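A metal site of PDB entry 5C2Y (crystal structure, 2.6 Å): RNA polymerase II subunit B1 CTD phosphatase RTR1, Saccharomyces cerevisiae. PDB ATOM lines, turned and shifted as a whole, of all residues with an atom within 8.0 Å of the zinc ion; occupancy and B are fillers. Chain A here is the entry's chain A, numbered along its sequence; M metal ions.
The side-chain sulfur (SG) of Cys 117 sits close to the side-chain hydroxyl (OG) of Ser 118 (3.1 Å).
N of Lys 85 lies close to SG of Cys 83, at 3.2 Å.
The backbone carbonyl oxygen (O) of Cys 78 lies within hydrogen-bond range of the guanidinium group (NH1) of Arg 72 (2.5 Å).
OG of Ser 118 lies within hydrogen-bond range of N of His 121 (3.4 Å).
The backbone carbonyl oxygen (O) of Cys 83 is in hydrogen-bond range of the guanidinium group (NH1) of Arg 72.
The backbone NH (N) of Cys 78 sits at hydrogen-bond distance from the backbone carbonyl oxygen (O) of Lys 85 (2.7 Å).
Four residues have an atom within 4 Å of the zinc ion: Cys 78, Cys 83, Cys 117 and His 121.
The zinc ion is bound by a ring nitrogen (ND1) of His 121 (2.1 Å), the side-chain sulfur (SG) of Cys 83 (2.2 Å), the side-chain sulfur (SG) of Cys 117 (2.3 Å) and the side-chain sulfur (SG) of Cys 78 (2.4 Å).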
ATOM      1  N   ARG A  72       8.194   9.245  32.598  1.00  0.00           N
ATOM      2  CA  ARG A  72       9.352   8.767  31.825  1.00  0.00           C
ATOM      3  C   ARG A  72      10.494   8.350  32.756  1.00  0.00           C
ATOM      4  O   ARG A  72      11.032   7.250  32.642  1.00  0.00           O
ATOM      5  CB  ARG A  72       9.879   9.835  30.860  1.00  0.00           C
ATOM      6  CG  ARG A  72       8.971  10.298  29.726  1.00  0.00           C
ATOM      7  CD  ARG A  72       9.803  10.924  28.607  1.00  0.00           C
ATOM      8  NE  ARG A  72       9.827  10.030  27.458  1.00  0.00           N
ATOM      9  CZ  ARG A  72      10.893   9.801  26.710  1.00  0.00           C
ATOM     10  NH1 ARG A  72      12.037  10.388  26.992  1.00  0.00           N
ATOM     11  NH2 ARG A  72      10.800   8.955  25.683  1.00  0.00           N
ATOM     12  N   ARG A  77      13.697   6.730  31.821  1.00  0.00           N
ATOM     13  CA  ARG A  77      13.968   7.402  30.548  1.00  0.00           C
ATOM     14  C   ARG A  77      14.220   8.887  30.736  1.00  0.00           C
ATOM     15  O   ARG A  77      13.631   9.499  31.617  1.00  0.00           O
ATOM     16  CB  ARG A  77      12.825   7.198  29.573  1.00  0.00           C
ATOM     17  CG  ARG A  77      12.372   5.776  29.488  1.00  0.00           C
ATOM     18  CD  ARG A  77      11.485   5.557  28.301  1.00  0.00           C
ATOM     19  NE  ARG A  77      12.239   5.756  27.072  1.00  0.00           N
ATOM     20  CZ  ARG A  77      12.719   4.761  26.329  1.00  0.00           C
ATOM     21  NH1 ARG A  77      12.494   3.495  26.670  1.00  0.00           N
ATOM     22  NH2 ARG A  77      13.411   5.045  25.223  1.00  0.00           N
ATOM     23  N   CYS A  78      15.088   9.459  29.915  1.00  0.00           N
ATOM     24  CA  CYS A  78      15.310  10.909  29.870  1.00  0.00           C
ATOM     25  C   CYS A  78      13.965  11.646  29.789  1.00  0.00           C
ATOM     26  O   CYS A  78      13.034  11.205  29.125  1.00  0.00           O
ATOM     27  CB  CYS A  78      16.178  11.258  28.668  1.00  0.00           C
ATOM     28  SG  CYS A  78      16.698  12.984  28.533  1.00  0.00           S
ATOM     29  N   GLY A  79      13.844  12.755  30.496  1.00  0.00           N
ATOM     30  CA  GLY A  79      12.560  13.435  30.555  1.00  0.00           C
ATOM     31  C   GLY A  79      12.048  13.921  29.209  1.00  0.00           C
ATOM     32  O   GLY A  79      10.828  13.946  28.985  1.00  0.00           O
ATOM     33  N   TYR A  80      12.965  14.294  28.325  1.00  0.00           N
ATOM     34  CA  TYR A  80      12.620  14.880  27.025  1.00  0.00           C
ATOM     35  C   TYR A  80      12.067  13.802  26.106  1.00  0.00           C
ATOM     36  O   TYR A  80      12.715  12.779  25.905  1.00  0.00           O
ATOM     37  CB  TYR A  80      13.856  15.545  26.420  1.00  0.00           C
ATOM     38  CG  TYR A  80      13.637  16.492  25.243  1.00  0.00           C
ATOM     39  CD1 TYR A  80      12.654  17.468  25.284  1.00  0.00           C
ATOM     40  CD2 TYR A  80      14.458  16.439  24.131  1.00  0.00           C
ATOM     41  CE1 TYR A  80      12.484  18.344  24.231  1.00  0.00           C
ATOM     42  CE2 TYR A  80      14.289  17.302  23.083  1.00  0.00           C
ATOM     43  CZ  TYR A  80      13.309  18.252  23.134  1.00  0.00           C
ATOM     44  OH  TYR A  80      13.157  19.112  22.075  1.00  0.00           O
ATOM     45  N   PRO A  81      10.876  14.023  25.522  1.00  0.00           N
ATOM     46  CA  PRO A  81      10.266  12.890  24.801  1.00  0.00           C
ATOM     47  C   PRO A  81      10.986  12.426  23.524  1.00  0.00           C
ATOM     48  O   PRO A  81      10.615  11.370  23.012  1.00  0.00           O
ATOM     49  CB  PRO A  81       8.858  13.412  24.460  1.00  0.00           C
ATOM     50  CG  PRO A  81       8.567  14.426  25.512  1.00  0.00           C
ATOM     51  CD  PRO A  81       9.904  15.093  25.775  1.00  0.00           C
ATOM     52  N   LEU A  82      11.976  13.159  23.027  1.00  0.00           N
ATOM     53  CA  LEU A  82      12.682  12.724  21.813  1.00  0.00           C
ATOM     54  C   LEU A  82      13.840  11.801  22.161  1.00  0.00           C
ATOM     55  O   LEU A  82      14.410  11.177  21.272  1.00  0.00           O
ATOM     56  CB  LEU A  82      13.189  13.916  21.006  1.00  0.00           C
ATOM     57  CG  LEU A  82      12.212  14.841  20.243  1.00  0.00           C
ATOM     58  CD1 LEU A  82      12.869  16.126  19.797  1.00  0.00           C
ATOM     59  CD2 LEU A  82      11.623  14.147  19.042  1.00  0.00           C
ATOM     60  N   CYS A  83      14.171  11.705  23.442  1.00  0.00           N
ATOM     61  CA  CYS A  83      15.378  10.983  23.871  1.00  0.00           C
ATOM     62  C   CYS A  83      15.076   9.601  24.412  1.00  0.00           C
ATOM     63  O   CYS A  83      14.215   9.460  25.274  1.00  0.00           O
ATOM     64  CB  CYS A  83      16.117  11.761  24.951  1.00  0.00           C
ATOM     65  SG  CYS A  83      17.619  10.929  25.516  1.00  0.00           S
ATOM     66  N   GLY A  84      15.815   8.610  23.942  1.00  0.00           N
ATOM     67  CA  GLY A  84      15.645   7.244  24.388  1.00  0.00           C
ATOM     68  C   GLY A  84      16.686   6.785  25.395  1.00  0.00           C
ATOM     69  O   GLY A  84      16.717   5.636  25.801  1.00  0.00           O
ATOM     70  N   LYS A  85      17.569   7.698  25.794  1.00  0.00           N
ATOM     71  CA  LYS A  85      18.530   7.399  26.846  1.00  0.00           C
ATOM     72  C   LYS A  85      17.873   7.505  28.223  1.00  0.00           C
ATOM     73  O   LYS A  85      16.732   7.950  28.363  1.00  0.00           O
ATOM     74  CB  LYS A  85      19.728   8.351  26.769  1.00  0.00           C
ATOM     75  CG  LYS A  85      20.667   8.165  25.591  1.00  0.00           C
ATOM     76  CD  LYS A  85      21.510   9.430  25.371  1.00  0.00           C
ATOM     77  CE  LYS A  85      22.963   9.262  25.737  1.00  0.00           C
ATOM     78  NZ  LYS A  85      23.628   8.272  24.835  1.00  0.00           N
ATOM     79  N   SER A  86      18.599   7.086  29.259  1.00  0.00           N
ATOM     80  CA  SER A  86      18.087   7.171  30.603  1.00  0.00           C
ATOM     81  C   SER A  86      18.698   8.412  31.266  1.00  0.00           C
ATOM     82  O   SER A  86      19.631   8.992  30.719  1.00  0.00           O
ATOM     83  CB  SER A  86      18.430   5.918  31.384  1.00  0.00           C
ATOM     84  OG  SER A  86      19.652   6.100  32.067  1.00  0.00           O
ATOM     85  N   PRO A  87      18.139   8.836  32.412  1.00  0.00           N
ATOM     86  CA  PRO A  87      18.755   9.952  33.146  1.00  0.00           C
ATOM     87  C   PRO A  87      20.188   9.608  33.557  1.00  0.00           C
ATOM     88  O   PRO A  87      20.527   8.432  33.597  1.00  0.00           O
ATOM     89  CB  PRO A  87      17.842  10.139  34.361  1.00  0.00           C
ATOM     90  CG  PRO A  87      16.530   9.638  33.902  1.00  0.00           C
ATOM     91  CD  PRO A  87      16.829   8.477  32.984  1.00  0.00           C
ATOM     92  N   GLU A  88      21.038  10.596  33.837  1.00  0.00           N
ATOM     93  CA  GLU A  88      22.418  10.272  34.148  1.00  0.00           C
ATOM     94  C   GLU A  88      22.550   9.746  35.570  1.00  0.00           C
ATOM     95  O   GLU A  88      23.336   8.832  35.835  1.00  0.00           O
ATOM     96  CB  GLU A  88      23.314  11.502  33.941  1.00  0.00           C
ATOM     97  CG  GLU A  88      24.781  11.261  34.272  1.00  0.00           C
ATOM     98  CD  GLU A  88      25.422  10.154  33.450  1.00  0.00           C
ATOM     99  OE1 GLU A  88      25.054   9.987  32.264  1.00  0.00           O
ATOM    100  OE2 GLU A  88      26.301   9.440  33.988  1.00  0.00           O
ATOM    101  N   HIS A 115      16.988  13.935  36.142  1.00  0.00           N
ATOM    102  CA  HIS A 115      15.791  13.895  35.303  1.00  0.00           C
ATOM    103  C   HIS A 115      16.058  13.719  33.798  1.00  0.00           C
ATOM    104  O   HIS A 115      15.171  13.319  33.027  1.00  0.00           O
ATOM    105  CB  HIS A 115      14.968  15.175  35.531  1.00  0.00           C
ATOM    106  CG  HIS A 115      14.597  15.391  36.965  1.00  0.00           C
ATOM    107  ND1 HIS A 115      13.708  14.578  37.628  1.00  0.00           N
ATOM    108  CD2 HIS A 115      15.052  16.288  37.868  1.00  0.00           C
ATOM    109  CE1 HIS A 115      13.599  14.988  38.884  1.00  0.00           C
ATOM    110  NE2 HIS A 115      14.406  16.016  39.057  1.00  0.00           N
ATOM    111  N   TYR A 116      17.291  14.013  33.378  1.00  0.00           N
ATOM    112  CA  TYR A 116      17.635  13.994  31.952  1.00  0.00           C
ATOM    113  C   TYR A 116      19.006  13.394  31.718  1.00  0.00           C
ATOM    114  O   TYR A 116      19.793  13.235  32.642  1.00  0.00           O
ATOM    115  CB  TYR A 116      17.573  15.401  31.371  1.00  0.00           C
ATOM    116  CG  TYR A 116      16.253  16.106  31.568  1.00  0.00           C
ATOM    117  CD1 TYR A 116      15.173  15.867  30.729  1.00  0.00           C
ATOM    118  CD2 TYR A 116      16.071  16.992  32.613  1.00  0.00           C
ATOM    119  CE1 TYR A 116      13.981  16.511  30.931  1.00  0.00           C
ATOM    120  CE2 TYR A 116      14.888  17.635  32.809  1.00  0.00           C
ATOM    121  CZ  TYR A 116      13.845  17.393  31.972  1.00  0.00           C
ATOM    122  OH  TYR A 116      12.665  18.051  32.188  1.00  0.00           O
ATOM    123  N   CYS A 117      19.291  13.036  30.476  1.00  0.00           N
ATOM    124  CA  CYS A 117      20.559  12.422  30.129  1.00  0.00           C
ATOM    125  C   CYS A 117      21.670  13.457  30.138  1.00  0.00           C
ATOM    126  O   CYS A 117      22.851  13.105  30.179  1.00  0.00           O
ATOM    127  CB  CYS A 117      20.484  11.765  28.745  1.00  0.00           C
ATOM    128  SG  CYS A 117      20.374  12.946  27.373  1.00  0.00           S
ATOM    129  N   SER A 118      21.289  14.731  30.086  1.00  0.00           N
ATOM    130  CA  SER A 118      22.248  15.827  29.948  1.00  0.00           C
ATOM    131  C   SER A 118      21.592  17.172  30.228  1.00  0.00           C
ATOM    132  O   SER A 118      20.363  17.296  30.257  1.00  0.00           O
ATOM    133  CB  SER A 118      22.825  15.821  28.557  1.00  0.00           C
ATOM    134  OG  SER A 118      21.748  15.760  27.647  1.00  0.00           O
ATOM    135  N   LYS A 119      22.419  18.199  30.414  1.00  0.00           N
ATOM    136  CA  LYS A 119      21.859  19.515  30.608  1.00  0.00           C
ATOM    137  C   LYS A 119      21.206  19.933  29.321  1.00  0.00           C
ATOM    138  O   LYS A 119      20.175  20.582  29.328  1.00  0.00           O
ATOM    139  CB  LYS A 119      22.920  20.545  31.029  1.00  0.00           C
ATOM    140  CG  LYS A 119      22.254  21.750  31.650  1.00  0.00           C
ATOM    141  CD  LYS A 119      23.206  22.792  32.194  1.00  0.00           C
ATOM    142  CE  LYS A 119      22.407  23.967  32.750  1.00  0.00           C
ATOM    143  NZ  LYS A 119      23.278  25.031  33.316  1.00  0.00           N
ATOM    144  N   PHE A 120      21.783  19.540  28.195  1.00  0.00           N
ATOM    145  CA  PHE A 120      21.221  19.914  26.907  1.00  0.00           C
ATOM    146  C   PHE A 120      19.748  19.503  26.801  1.00  0.00           C
ATOM    147  O   PHE A 120      18.887  20.329  26.481  1.00  0.00           O
ATOM    148  CB  PHE A 120      22.018  19.314  25.755  1.00  0.00           C
ATOM    149  CG  PHE A 120      21.474  19.696  24.422  1.00  0.00           C
ATOM    150  CD1 PHE A 120      21.467  21.033  24.027  1.00  0.00           C
ATOM    151  CD2 PHE A 120      20.927  18.749  23.573  1.00  0.00           C
ATOM    152  CE1 PHE A 120      20.950  21.406  22.790  1.00  0.00           C
ATOM    153  CE2 PHE A 120      20.411  19.109  22.340  1.00  0.00           C
ATOM    154  CZ  PHE A 120      20.417  20.441  21.947  1.00  0.00           C
ATOM    155  N   HIS A 121      19.447  18.244  27.101  1.00  0.00           N
ATOM    156  CA  HIS A 121      18.051  17.805  27.062  1.00  0.00           C
ATOM    157  C   HIS A 121      17.174  18.387  28.189  1.00  0.00           C
ATOM    158  O   HIS A 121      15.984  18.582  27.989  1.00  0.00           O
ATOM    159  CB  HIS A 121      17.990  16.291  27.053  1.00  0.00           C
ATOM    160  CG  HIS A 121      18.145  15.709  25.688  1.00  0.00           C
ATOM    161  ND1 HIS A 121      18.367  14.372  25.466  1.00  0.00           N
ATOM    162  CD2 HIS A 121      18.117  16.306  24.475  1.00  0.00           C
ATOM    163  CE1 HIS A 121      18.477  14.164  24.166  1.00  0.00           C
ATOM    164  NE2 HIS A 121      18.330  15.318  23.535  1.00  0.00           N
ATOM    165  N   PHE A 122      17.766  18.690  29.353  1.00  0.00           N
ATOM    166  CA  PHE A 122      17.048  19.473  30.366  1.00  0.00           C
ATOM    167  C   PHE A 122      16.540  20.781  29.778  1.00  0.00           C
ATOM    168  O   PHE A 122      15.389  21.161  29.991  1.00  0.00           O
ATOM    169  CB  PHE A 122      17.941  19.771  31.580  1.00  0.00           C
ATOM    170  CG  PHE A 122      17.459  20.935  32.390  1.00  0.00           C
ATOM    171  CD1 PHE A 122      16.322  20.838  33.158  1.00  0.00           C
ATOM    172  CD2 PHE A 122      18.122  22.147  32.364  1.00  0.00           C
ATOM    173  CE1 PHE A 122      15.853  21.931  33.896  1.00  0.00           C
ATOM    174  CE2 PHE A 122      17.662  23.239  33.097  1.00  0.00           C
ATOM    175  CZ  PHE A 122      16.521  23.134  33.861  1.00  0.00           C
HETATM  176 ZN    ZN M   1      18.192  12.697  26.724  1.00  0.00          ZN
